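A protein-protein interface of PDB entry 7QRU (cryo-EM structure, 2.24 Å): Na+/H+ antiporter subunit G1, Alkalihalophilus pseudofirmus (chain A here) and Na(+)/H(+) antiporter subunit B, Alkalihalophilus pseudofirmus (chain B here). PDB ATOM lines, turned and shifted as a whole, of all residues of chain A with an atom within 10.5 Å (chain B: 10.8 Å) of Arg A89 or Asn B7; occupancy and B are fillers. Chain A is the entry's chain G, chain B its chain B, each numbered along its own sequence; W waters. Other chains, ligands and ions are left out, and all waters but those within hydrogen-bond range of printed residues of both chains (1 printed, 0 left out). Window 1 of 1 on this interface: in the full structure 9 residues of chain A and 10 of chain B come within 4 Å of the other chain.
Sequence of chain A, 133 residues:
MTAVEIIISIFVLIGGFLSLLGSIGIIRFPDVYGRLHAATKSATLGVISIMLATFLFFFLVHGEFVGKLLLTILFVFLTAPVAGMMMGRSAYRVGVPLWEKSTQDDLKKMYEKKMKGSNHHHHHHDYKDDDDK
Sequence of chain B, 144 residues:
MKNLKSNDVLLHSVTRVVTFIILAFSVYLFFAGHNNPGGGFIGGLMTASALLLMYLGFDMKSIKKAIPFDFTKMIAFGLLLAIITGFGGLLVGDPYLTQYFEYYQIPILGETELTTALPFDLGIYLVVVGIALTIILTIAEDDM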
ATOM      1  N   VAL A  32     -22.184  18.197  10.760  1.00  0.00           N
ATOM      2  CA  VAL A  32     -21.864  19.511  10.293  1.00  0.00           C
ATOM      3  C   VAL A  32     -22.778  20.509  11.018  1.00  0.00           C
ATOM      4  O   VAL A  32     -22.367  21.687  11.164  1.00  0.00           O
ATOM      5  CB  VAL A  32     -21.986  19.629   8.762  1.00  0.00           C
ATOM      6  CG1 VAL A  32     -23.411  19.420   8.315  1.00  0.00           C
ATOM      7  CG2 VAL A  32     -21.496  20.967   8.218  1.00  0.00           C
ATOM      8  N   TYR A  33     -23.987  20.116  11.439  1.00  0.00           N
ATOM      9  CA  TYR A  33     -24.932  21.059  12.066  1.00  0.00           C
ATOM     10  C   TYR A  33     -24.432  21.547  13.429  1.00  0.00           C
ATOM     11  O   TYR A  33     -24.494  22.730  13.656  1.00  0.00           O
ATOM     12  CB  TYR A  33     -26.291  20.416  12.241  1.00  0.00           C
ATOM     13  CG  TYR A  33     -26.759  19.881  10.915  1.00  0.00           C
ATOM     14  CD1 TYR A  33     -27.148  20.761   9.919  1.00  0.00           C
ATOM     15  CD2 TYR A  33     -26.729  18.512  10.628  1.00  0.00           C
ATOM     16  CE1 TYR A  33     -27.388  20.326   8.625  1.00  0.00           C
ATOM     17  CE2 TYR A  33     -26.972  18.080   9.345  1.00  0.00           C
ATOM     18  CZ  TYR A  33     -27.435  18.972   8.386  1.00  0.00           C
ATOM     19  OH  TYR A  33     -27.680  18.452   7.145  1.00  0.00           O
ATOM     20  N   LEU A  36     -21.484  23.899  12.976  1.00  0.00           N
ATOM     21  CA  LEU A  36     -21.919  25.252  12.674  1.00  0.00           C
ATOM     22  C   LEU A  36     -22.204  25.963  14.000  1.00  0.00           C
ATOM     23  O   LEU A  36     -22.102  27.174  14.052  1.00  0.00           O
ATOM     24  CB  LEU A  36     -23.136  25.281  11.714  1.00  0.00           C
ATOM     25  CG  LEU A  36     -22.766  25.095  10.279  1.00  0.00           C
ATOM     26  CD1 LEU A  36     -23.946  24.705   9.500  1.00  0.00           C
ATOM     27  CD2 LEU A  36     -22.131  26.324   9.728  1.00  0.00           C
ATOM     28  N   THR A  40     -20.265  29.539  13.899  1.00  0.00           N
ATOM     29  CA  THR A  40     -21.087  30.719  14.056  1.00  0.00           C
ATOM     30  C   THR A  40     -20.949  31.433  15.404  1.00  0.00           C
ATOM     31  O   THR A  40     -21.103  32.642  15.415  1.00  0.00           O
ATOM     32  CB  THR A  40     -22.515  30.308  13.758  1.00  0.00           C
ATOM     33  OG1 THR A  40     -22.318  29.659  12.480  1.00  0.00           O
ATOM     34  CG2 THR A  40     -23.479  31.465  13.648  1.00  0.00           C
ATOM     35  N   PRO A  81     -24.584  34.954  11.138  1.00  0.00           N
ATOM     36  CA  PRO A  81     -25.813  34.181  11.075  1.00  0.00           C
ATOM     37  C   PRO A  81     -26.192  33.762   9.664  1.00  0.00           C
ATOM     38  O   PRO A  81     -26.563  32.622   9.479  1.00  0.00           O
ATOM     39  CB  PRO A  81     -26.838  35.116  11.721  1.00  0.00           C
ATOM     40  CG  PRO A  81     -25.984  35.928  12.631  1.00  0.00           C
ATOM     41  CD  PRO A  81     -24.759  36.243  11.804  1.00  0.00           C
ATOM     42  N   VAL A  82     -26.190  34.669   8.708  1.00  0.00           N
ATOM     43  CA  VAL A  82     -26.613  34.280   7.383  1.00  0.00           C
ATOM     44  C   VAL A  82     -25.637  33.244   6.799  1.00  0.00           C
ATOM     45  O   VAL A  82     -26.009  32.394   6.054  1.00  0.00           O
ATOM     46  CB  VAL A  82     -26.798  35.506   6.457  1.00  0.00           C
ATOM     47  CG1 VAL A  82     -25.627  36.397   6.312  1.00  0.00           C
ATOM     48  CG2 VAL A  82     -27.139  35.027   5.080  1.00  0.00           C
ATOM     49  N   ALA A  83     -24.342  33.386   6.995  1.00  0.00           N
ATOM     50  CA  ALA A  83     -23.440  32.398   6.450  1.00  0.00           C
ATOM     51  C   ALA A  83     -23.741  31.025   7.053  1.00  0.00           C
ATOM     52  O   ALA A  83     -23.761  30.052   6.342  1.00  0.00           O
ATOM     53  CB  ALA A  83     -22.068  32.776   6.792  1.00  0.00           C
ATOM     54  N   GLY A  84     -23.907  30.914   8.358  1.00  0.00           N
ATOM     55  CA  GLY A  84     -24.163  29.622   8.949  1.00  0.00           C
ATOM     56  C   GLY A  84     -25.494  29.082   8.444  1.00  0.00           C
ATOM     57  O   GLY A  84     -25.644  27.897   8.317  1.00  0.00           O
ATOM     58  N   MET A  85     -26.460  29.934   8.185  1.00  0.00           N
ATOM     59  CA  MET A  85     -27.735  29.462   7.690  1.00  0.00           C
ATOM     60  C   MET A  85     -27.598  28.901   6.270  1.00  0.00           C
ATOM     61  O   MET A  85     -28.143  27.856   5.973  1.00  0.00           O
ATOM     62  CB  MET A  85     -28.772  30.580   7.640  1.00  0.00           C
ATOM     63  CG  MET A  85     -30.007  29.990   6.976  1.00  0.00           C
ATOM     64  SD  MET A  85     -31.358  31.027   6.600  1.00  0.00           S
ATOM     65  CE  MET A  85     -32.041  31.337   8.240  1.00  0.00           C
ATOM     66  N   MET A  86     -26.893  29.586   5.396  1.00  0.00           N
ATOM     67  CA  MET A  86     -26.712  29.176   4.045  1.00  0.00           C
ATOM     68  C   MET A  86     -25.842  27.931   4.003  1.00  0.00           C
ATOM     69  O   MET A  86     -26.135  27.128   3.204  1.00  0.00           O
ATOM     70  CB  MET A  86     -26.022  30.292   3.260  1.00  0.00           C
ATOM     71  CG  MET A  86     -26.862  31.516   2.980  1.00  0.00           C
ATOM     72  SD  MET A  86     -28.170  31.208   1.875  1.00  0.00           S
ATOM     73  CE  MET A  86     -29.486  31.060   3.103  1.00  0.00           C
ATOM     74  N   MET A  87     -24.826  27.747   4.832  1.00  0.00           N
ATOM     75  CA  MET A  87     -24.070  26.510   4.955  1.00  0.00           C
ATOM     76  C   MET A  87     -24.872  25.384   5.618  1.00  0.00           C
ATOM     77  O   MET A  87     -24.721  24.264   5.240  1.00  0.00           O
ATOM     78  CB  MET A  87     -22.694  26.679   5.676  1.00  0.00           C
ATOM     79  CG  MET A  87     -21.804  27.620   4.865  1.00  0.00           C
ATOM     80  SD  MET A  87     -20.174  28.053   5.598  1.00  0.00           S
ATOM     81  CE  MET A  87     -20.644  28.527   7.260  1.00  0.00           C
ATOM     82  N   GLY A  88     -25.735  25.616   6.541  1.00  0.00           N
ATOM     83  CA  GLY A  88     -26.393  24.490   7.126  1.00  0.00           C
ATOM     84  C   GLY A  88     -27.531  24.059   6.268  1.00  0.00           C
ATOM     85  O   GLY A  88     -27.765  22.868   6.190  1.00  0.00           O
ATOM     86  N   ARG A  89     -28.207  25.026   5.593  1.00  0.00           N
ATOM     87  CA  ARG A  89     -29.373  24.672   4.802  1.00  0.00           C
ATOM     88  C   ARG A  89     -28.918  24.026   3.494  1.00  0.00           C
ATOM     89  O   ARG A  89     -29.505  23.124   3.056  1.00  0.00           O
ATOM     90  CB  ARG A  89     -30.167  25.886   4.459  1.00  0.00           C
ATOM     91  CG  ARG A  89     -31.470  25.547   3.742  1.00  0.00           C
ATOM     92  CD  ARG A  89     -32.328  26.772   3.811  1.00  0.00           C
ATOM     93  NE  ARG A  89     -31.714  27.659   2.872  1.00  0.00           N
ATOM     94  CZ  ARG A  89     -32.231  28.832   2.611  1.00  0.00           C
ATOM     95  NH1 ARG A  89     -33.245  29.273   3.360  1.00  0.00           N
ATOM     96  NH2 ARG A  89     -31.733  29.519   1.604  1.00  0.00           N
ATOM     97  N   SER A  90     -27.825  24.471   2.905  1.00  0.00           N
ATOM     98  CA  SER A  90     -27.252  23.824   1.776  1.00  0.00           C
ATOM     99  C   SER A  90     -26.904  22.366   2.077  1.00  0.00           C
ATOM    100  O   SER A  90     -27.183  21.503   1.264  1.00  0.00           O
ATOM    101  CB  SER A  90     -25.964  24.607   1.339  1.00  0.00           C
ATOM    102  OG  SER A  90     -25.118  23.815   0.531  1.00  0.00           O
ATOM    103  N   ALA A  91     -26.306  22.086   3.242  1.00  0.00           N
ATOM    104  CA  ALA A  91     -25.990  20.725   3.659  1.00  0.00           C
ATOM    105  C   ALA A  91     -27.236  19.887   3.751  1.00  0.00           C
ATOM    106  O   ALA A  91     -27.244  18.757   3.300  1.00  0.00           O
ATOM    107  CB  ALA A  91     -25.336  20.727   4.984  1.00  0.00           C
ATOM    108  N   TYR A  92     -28.297  20.458   4.363  1.00  0.00           N
ATOM    109  CA  TYR A  92     -29.513  19.654   4.603  1.00  0.00           C
ATOM    110  C   TYR A  92     -30.164  19.329   3.232  1.00  0.00           C
ATOM    111  O   TYR A  92     -30.627  18.233   3.025  1.00  0.00           O
ATOM    112  CB  TYR A  92     -30.441  20.387   5.577  1.00  0.00           C
ATOM    113  CG  TYR A  92     -31.579  19.528   6.080  1.00  0.00           C
ATOM    114  CD1 TYR A  92     -32.772  19.393   5.399  1.00  0.00           C
ATOM    115  CD2 TYR A  92     -31.431  18.790   7.199  1.00  0.00           C
ATOM    116  CE1 TYR A  92     -33.756  18.548   5.813  1.00  0.00           C
ATOM    117  CE2 TYR A  92     -32.423  17.968   7.677  1.00  0.00           C
ATOM    118  CZ  TYR A  92     -33.591  17.837   6.971  1.00  0.00           C
ATOM    119  OH  TYR A  92     -34.596  17.033   7.434  1.00  0.00           O
ATOM    120  N   ARG A  93     -30.206  20.290   2.309  1.00  0.00           N
ATOM    121  CA  ARG A  93     -30.798  20.053   1.050  1.00  0.00           C
ATOM    122  C   ARG A  93     -29.963  19.029   0.249  1.00  0.00           C
ATOM    123  O   ARG A  93     -30.500  18.257  -0.508  1.00  0.00           O
ATOM    124  CB  ARG A  93     -30.927  21.383   0.305  1.00  0.00           C
ATOM    125  CG  ARG A  93     -31.965  22.347   0.842  1.00  0.00           C
ATOM    126  CD  ARG A  93     -31.944  23.626   0.168  1.00  0.00           C
ATOM    127  NE  ARG A  93     -33.008  24.499   0.600  1.00  0.00           N
ATOM    128  CZ  ARG A  93     -33.132  25.795   0.291  1.00  0.00           C
ATOM    129  NH1 ARG A  93     -32.184  26.434  -0.371  1.00  0.00           N
ATOM    130  NH2 ARG A  93     -34.182  26.464   0.728  1.00  0.00           N
ATOM    131  N   VAL A  94     -28.655  19.076   0.334  1.00  0.00           N
ATOM    132  CA  VAL A  94     -27.782  18.199  -0.452  1.00  0.00           C
ATOM    133  C   VAL A  94     -27.816  16.768   0.123  1.00  0.00           C
ATOM    134  O   VAL A  94     -27.346  15.851  -0.498  1.00  0.00           O
ATOM    135  CB  VAL A  94     -26.350  18.782  -0.544  1.00  0.00           C
ATOM    136  CG1 VAL A  94     -25.466  18.300   0.556  1.00  0.00           C
ATOM    137  CG2 VAL A  94     -25.784  18.494  -1.884  1.00  0.00           C
ATOM    138  N   GLY A  95     -28.439  16.610   1.273  1.00  0.00           N
ATOM    139  CA  GLY A  95     -28.671  15.335   1.878  1.00  0.00           C
ATOM    140  C   GLY A  95     -27.727  14.978   3.015  1.00  0.00           C
ATOM    141  O   GLY A  95     -27.745  13.799   3.450  1.00  0.00           O
ATOM    142  N   VAL A  96     -26.833  15.885   3.429  1.00  0.00           N
ATOM    143  CA  VAL A  96     -25.972  15.556   4.580  1.00  0.00           C
ATOM    144  C   VAL A  96     -26.858  15.213   5.775  1.00  0.00           C
ATOM    145  O   VAL A  96     -27.745  16.012   6.070  1.00  0.00           O
ATOM    146  CB  VAL A  96     -25.003  16.690   4.929  1.00  0.00           C
ATOM    147  CG1 VAL A  96     -24.337  16.366   6.196  1.00  0.00           C
ATOM    148  CG2 VAL A  96     -24.070  16.980   3.754  1.00  0.00           C
ATOM    149  N   PRO A  97     -26.832  13.991   6.367  1.00  0.00           N
ATOM    150  CA  PRO A  97     -27.808  13.589   7.378  1.00  0.00           C
ATOM    151  C   PRO A  97     -27.491  14.225   8.714  1.00  0.00           C
ATOM    152  O   PRO A  97     -26.316  14.495   9.065  1.00  0.00           O
ATOM    153  CB  PRO A  97     -27.522  12.089   7.618  1.00  0.00           C
ATOM    154  CG  PRO A  97     -26.652  11.716   6.489  1.00  0.00           C
ATOM    155  CD  PRO A  97     -25.852  12.932   6.182  1.00  0.00           C
ATOM    156  N   LEU A  98     -28.529  14.390   9.505  1.00  0.00           N
ATOM    157  CA  LEU A  98     -28.308  14.815  10.887  1.00  0.00           C
ATOM    158  C   LEU A  98     -27.576  13.656  11.598  1.00  0.00           C
ATOM    159  O   LEU A  98     -27.592  12.522  11.122  1.00  0.00           O
ATOM    160  CB  LEU A  98     -29.671  15.067  11.526  1.00  0.00           C
ATOM    161  CG  LEU A  98     -30.049  16.485  11.823  1.00  0.00           C
ATOM    162  CD1 LEU A  98     -30.160  17.269  10.612  1.00  0.00           C
ATOM    163  CD2 LEU A  98     -31.393  16.499  12.440  1.00  0.00           C
ATOM    164  N   LEU A 107     -37.866  19.737   9.876  1.00  0.00           N
ATOM    165  CA  LEU A 107     -37.503  20.243   8.580  1.00  0.00           C
ATOM    166  C   LEU A 107     -37.634  19.156   7.509  1.00  0.00           C
ATOM    167  O   LEU A 107     -37.809  19.441   6.353  1.00  0.00           O
ATOM    168  CB  LEU A 107     -36.059  20.762   8.710  1.00  0.00           C
ATOM    169  CG  LEU A 107     -35.540  21.475   7.459  1.00  0.00           C
ATOM    170  CD1 LEU A 107     -36.378  22.730   7.120  1.00  0.00           C
ATOM    171  CD2 LEU A 107     -34.162  21.903   7.673  1.00  0.00           C
ATOM    172  N   MET A 110     -41.261  19.430   5.983  1.00  0.00           N
ATOM    173  CA  MET A 110     -41.289  20.548   5.055  1.00  0.00           C
ATOM    174  C   MET A 110     -40.625  20.158   3.734  1.00  0.00           C
ATOM    175  O   MET A 110     -41.252  20.307   2.684  1.00  0.00           O
ATOM    176  CB  MET A 110     -40.597  21.786   5.641  1.00  0.00           C
ATOM    177  CG  MET A 110     -40.985  23.064   4.946  1.00  0.00           C
ATOM    178  SD  MET A 110     -39.938  24.472   5.230  1.00  0.00           S
ATOM    179  CE  MET A 110     -38.693  24.191   3.992  1.00  0.00           C
ATOM    180  N   TYR A 111     -39.394  19.620   3.752  1.00  0.00           N
ATOM    181  CA  TYR A 111     -38.738  19.254   2.487  1.00  0.00           C
ATOM    182  C   TYR A 111     -39.352  18.005   1.835  1.00  0.00           C
ATOM    183  O   TYR A 111     -38.866  17.577   0.787  1.00  0.00           O
ATOM    184  CB  TYR A 111     -37.224  19.006   2.621  1.00  0.00           C
ATOM    185  CG  TYR A 111     -36.489  20.305   2.594  1.00  0.00           C
ATOM    186  CD1 TYR A 111     -36.329  20.970   1.399  1.00  0.00           C
ATOM    187  CD2 TYR A 111     -36.179  20.956   3.763  1.00  0.00           C
ATOM    188  CE1 TYR A 111     -35.808  22.240   1.365  1.00  0.00           C
ATOM    189  CE2 TYR A 111     -35.639  22.219   3.745  1.00  0.00           C
ATOM    190  CZ  TYR A 111     -35.458  22.864   2.549  1.00  0.00           C
ATOM    191  OH  TYR A 111     -34.861  24.100   2.522  1.00  0.00           O
ATOM    192  N   LYS B   5     -38.857  28.825  -4.565  1.00  0.00           N
ATOM    193  CA  LYS B   5     -38.506  27.494  -4.000  1.00  0.00           C
ATOM    194  C   LYS B   5     -37.623  27.616  -2.741  1.00  0.00           C
ATOM    195  O   LYS B   5     -37.822  26.821  -1.818  1.00  0.00           O
ATOM    196  CB  LYS B   5     -37.812  26.615  -5.048  1.00  0.00           C
ATOM    197  CG  LYS B   5     -37.643  25.155  -4.630  1.00  0.00           C
ATOM    198  CD  LYS B   5     -36.599  24.378  -5.408  1.00  0.00           C
ATOM    199  CE  LYS B   5     -36.292  23.035  -4.778  1.00  0.00           C
ATOM    200  NZ  LYS B   5     -35.468  22.190  -5.677  1.00  0.00           N
ATOM    201  N   SER B   6     -36.667  28.568  -2.670  1.00  0.00           N
ATOM    202  CA  SER B   6     -35.996  28.871  -1.408  1.00  0.00           C
ATOM    203  C   SER B   6     -36.459  30.216  -0.840  1.00  0.00           C
ATOM    204  O   SER B   6     -36.396  31.227  -1.537  1.00  0.00           O
ATOM    205  CB  SER B   6     -34.481  28.853  -1.553  1.00  0.00           C
ATOM    206  OG  SER B   6     -34.079  29.703  -2.591  1.00  0.00           O
ATOM    207  N   ASN B   7     -36.892  30.248   0.415  1.00  0.00           N
ATOM    208  CA  ASN B   7     -37.060  31.489   1.172  1.00  0.00           C
ATOM    209  C   ASN B   7     -35.685  32.080   1.522  1.00  0.00           C
ATOM    210  O   ASN B   7     -34.948  31.602   2.358  1.00  0.00           O
ATOM    211  CB  ASN B   7     -37.953  31.160   2.343  1.00  0.00           C
ATOM    212  CG  ASN B   7     -38.595  32.320   3.026  1.00  0.00           C
ATOM    213  OD1 ASN B   7     -38.027  33.381   3.117  1.00  0.00           O
ATOM    214  ND2 ASN B   7     -39.716  32.037   3.665  1.00  0.00           N
ATOM    215  N   ASP B   8     -35.335  33.139   0.812  1.00  0.00           N
ATOM    216  CA  ASP B   8     -34.087  33.867   0.973  1.00  0.00           C
ATOM    217  C   ASP B   8     -34.292  35.183   1.728  1.00  0.00           C
ATOM    218  O   ASP B   8     -33.522  36.100   1.564  1.00  0.00           O
ATOM    219  CB  ASP B   8     -33.526  34.131  -0.424  1.00  0.00           C
ATOM    220  CG  ASP B   8     -33.133  32.805  -1.084  1.00  0.00           C
ATOM    221  OD1 ASP B   8     -32.700  31.890  -0.329  1.00  0.00           O
ATOM    222  OD2 ASP B   8     -33.241  32.681  -2.353  1.00  0.00           O
ATOM    223  N   VAL B   9     -35.356  35.339   2.486  1.00  0.00           N
ATOM    224  CA  VAL B   9     -35.606  36.574   3.187  1.00  0.00           C
ATOM    225  C   VAL B   9     -34.341  37.080   3.922  1.00  0.00           C
ATOM    226  O   VAL B   9     -34.160  38.299   4.005  1.00  0.00           O
ATOM    227  CB  VAL B   9     -36.758  36.448   4.200  1.00  0.00           C
ATOM    228  CG1 VAL B   9     -36.437  35.481   5.321  1.00  0.00           C
ATOM    229  CG2 VAL B   9     -37.074  37.788   4.805  1.00  0.00           C
ATOM    230  N   LEU B  10     -33.568  36.196   4.563  1.00  0.00           N
ATOM    231  CA  LEU B  10     -32.410  36.643   5.319  1.00  0.00           C
ATOM    232  C   LEU B  10     -31.231  36.949   4.402  1.00  0.00           C
ATOM    233  O   LEU B  10     -30.576  37.941   4.593  1.00  0.00           O
ATOM    234  CB  LEU B  10     -32.049  35.613   6.381  1.00  0.00           C
ATOM    235  CG  LEU B  10     -30.792  35.849   7.194  1.00  0.00           C
ATOM    236  CD1 LEU B  10     -30.862  37.118   8.005  1.00  0.00           C
ATOM    237  CD2 LEU B  10     -30.573  34.650   8.117  1.00  0.00           C
ATOM    238  N   LEU B  11     -30.893  36.104   3.447  1.00  0.00           N
ATOM    239  CA  LEU B  11     -29.858  36.458   2.490  1.00  0.00           C
ATOM    240  C   LEU B  11     -30.168  37.762   1.737  1.00  0.00           C
ATOM    241  O   LEU B  11     -29.273  38.626   1.611  1.00  0.00           O
ATOM    242  CB  LEU B  11     -29.633  35.282   1.539  1.00  0.00           C
ATOM    243  CG  LEU B  11     -28.533  35.534   0.508  1.00  0.00           C
ATOM    244  CD1 LEU B  11     -27.261  35.833   1.169  1.00  0.00           C
ATOM    245  CD2 LEU B  11     -28.404  34.421  -0.430  1.00  0.00           C
ATOM    246  N   HIS B  12     -31.377  37.963   1.237  1.00  0.00           N
ATOM    247  CA  HIS B  12     -31.729  39.222   0.550  1.00  0.00           C
ATOM    248  C   HIS B  12     -31.688  40.443   1.440  1.00  0.00           C
ATOM    249  O   HIS B  12     -31.136  41.428   1.027  1.00  0.00           O
ATOM    250  CB  HIS B  12     -33.085  39.200  -0.105  1.00  0.00           C
ATOM    251  CG  HIS B  12     -33.230  38.188  -1.178  1.00  0.00           C
ATOM    252  ND1 HIS B  12     -32.199  37.532  -1.766  1.00  0.00           N
ATOM    253  CD2 HIS B  12     -34.368  37.900  -1.863  1.00  0.00           C
ATOM    254  CE1 HIS B  12     -32.709  36.763  -2.721  1.00  0.00           C
ATOM    255  NE2 HIS B  12     -34.054  37.008  -2.831  1.00  0.00           N
ATOM    256  N   SER B  13     -32.017  40.305   2.706  1.00  0.00           N
ATOM    257  CA  SER B  13     -31.940  41.412   3.647  1.00  0.00           C
ATOM    258  C   SER B  13     -30.515  41.825   3.943  1.00  0.00           C
ATOM    259  O   SER B  13     -30.163  42.960   3.861  1.00  0.00           O
ATOM    260  CB  SER B  13     -32.591  41.050   4.928  1.00  0.00           C
ATOM    261  OG  SER B  13     -34.021  41.022   4.706  1.00  0.00           O
ATOM    262  N   ARG B  16     -28.683  43.399   0.761  1.00  0.00           N
ATOM    263  CA  ARG B  16     -28.930  44.818   0.653  1.00  0.00           C
ATOM    264  C   ARG B  16     -28.107  45.666   1.634  1.00  0.00           C
ATOM    265  O   ARG B  16     -27.799  46.763   1.267  1.00  0.00           O
ATOM    266  CB  ARG B  16     -30.411  45.172   0.793  1.00  0.00           C
ATOM    267  CG  ARG B  16     -31.192  44.504  -0.305  1.00  0.00           C
ATOM    268  CD  ARG B  16     -32.670  44.734  -0.108  1.00  0.00           C
ATOM    269  NE  ARG B  16     -33.314  44.276  -1.343  1.00  0.00           N
ATOM    270  CZ  ARG B  16     -34.212  43.324  -1.359  1.00  0.00           C
ATOM    271  NH1 ARG B  16     -34.491  42.708  -0.209  1.00  0.00           N
ATOM    272  NH2 ARG B  16     -34.796  42.991  -2.505  1.00  0.00           N
ATOM    273  N   LEU B  56     -24.811  37.136  -6.722  1.00  0.00           N
ATOM    274  CA  LEU B  56     -24.893  35.947  -5.880  1.00  0.00           C
ATOM    275  C   LEU B  56     -26.152  35.891  -5.023  1.00  0.00           C
ATOM    276  O   LEU B  56     -26.610  34.837  -4.689  1.00  0.00           O
ATOM    277  CB  LEU B  56     -23.694  36.064  -4.952  1.00  0.00           C
ATOM    278  CG  LEU B  56     -22.896  34.824  -4.669  1.00  0.00           C
ATOM    279  CD1 LEU B  56     -22.572  34.119  -5.933  1.00  0.00           C
ATOM    280  CD2 LEU B  56     -21.610  35.245  -3.969  1.00  0.00           C
ATOM    281  N   GLY B  57     -26.480  37.029  -4.395  1.00  0.00           N
ATOM    282  CA  GLY B  57     -27.559  37.103  -3.453  1.00  0.00           C
ATOM    283  C   GLY B  57     -28.920  37.067  -4.131  1.00  0.00           C
ATOM    284  O   GLY B  57     -29.893  36.746  -3.446  1.00  0.00           O
ATOM    285  N   PHE B  58     -29.021  37.563  -5.384  1.00  0.00           N
ATOM    286  CA  PHE B  58     -30.304  37.693  -6.022  1.00  0.00           C
ATOM    287  C   PHE B  58     -30.263  36.805  -7.247  1.00  0.00           C
ATOM    288  O   PHE B  58     -30.105  35.607  -7.061  1.00  0.00           O
ATOM    289  CB  PHE B  58     -30.638  39.177  -6.194  1.00  0.00           C
ATOM    290  CG  PHE B  58     -30.949  39.933  -4.954  1.00  0.00           C
ATOM    291  CD1 PHE B  58     -29.956  40.471  -4.232  1.00  0.00           C
ATOM    292  CD2 PHE B  58     -32.230  40.066  -4.454  1.00  0.00           C
ATOM    293  CE1 PHE B  58     -30.234  41.101  -3.006  1.00  0.00           C
ATOM    294  CE2 PHE B  58     -32.489  40.773  -3.266  1.00  0.00           C
ATOM    295  CZ  PHE B  58     -31.505  41.327  -2.563  1.00  0.00           C
HETATM  296  O   HOH W   1     -36.487  27.943   2.171  1.00  0.00           O
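The backbone carbonyl oxygen of Asn B7 sits at hydrogen-bond distance from the guanidinium group of Arg A89 (3.1 Å). The side-chain carboxylate (OD1) of Asp B8 is in salt-bridge range of the guanidinium group (NH2) of Arg A89.
Of the 25 printed residues of chain A, 5 touch a printed residue of chain B. Of the 13 printed residues of chain B, 5 touch a printed residue of chain A. Hydrophobic or aromatic side chains of chain B within 4 Å of the printed part of chain A: Leu B10 and Leu B11. Among the printed residues, 6 pairs touch across the chains. Among the printed residues, Asp or Glu carboxylates within 4 Å of a Lys or Arg side-chain nitrogen of the other chain: Arg A89 with Asp B8 (3.2 Å).
Met A85 touches one residue of chain B. Of the printed residues of chain B, Met A86 touches Leu B11 (3.96 Å). No residue of chain B comes within 4 Å of Gly A88. Arg A89 touches just these residues of chain B: Asn B7 (3.1 Å) and Asp B8 (3.2 Å). No residue of chain B comes within 4 Å of Ser A90. Ala A91 touches none of the printed residues of chain B. Val A96 touches none of the printed residues of chain B. Met A110 touches none of the printed residues of chain B. Asn B7 touches one residue of chain A. Of the printed residues of chain A, Asp B8 touches Arg A89. Val B9 touches none of the printed residues of chain A. Printed residues of chain A within 4 Å of Leu B10: Met A85 (3.6 Å). Printed residues of chain A within 4 Å of Leu B11: Val A82 (3.995 Å) and Met A86 (3.96 Å). The nearest residue of chain A that does not touch Asn B7 is Arg A93 (4.7 Å).
The side-chain carboxylate (OD2) of Asp B8 is in hydrogen-bond range of the side-chain hydroxyl (OG) of Ser B6. The side-chain amide oxygen (OD1) of Asn B7 lies within hydrogen-bond range of the backbone NH (N) of Val B9. The guanidinium group of Arg A93 is in hydrogen-bond range of the side-chain hydroxyl of Tyr A111.
Water W1 bridges the backbone NH (N) of Asn B7 (2.9 Å) and the guanidinium group (NH2) of Arg A93 (3.1 Å).
Val A82 touches Leu B11 (CG2 to CD1, 3.995 Å). Leu B10 touches Met A85. Met A86 touches Leu B11. Ser B6 touches Arg A93 (CB to NH2, 3.3 Å).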
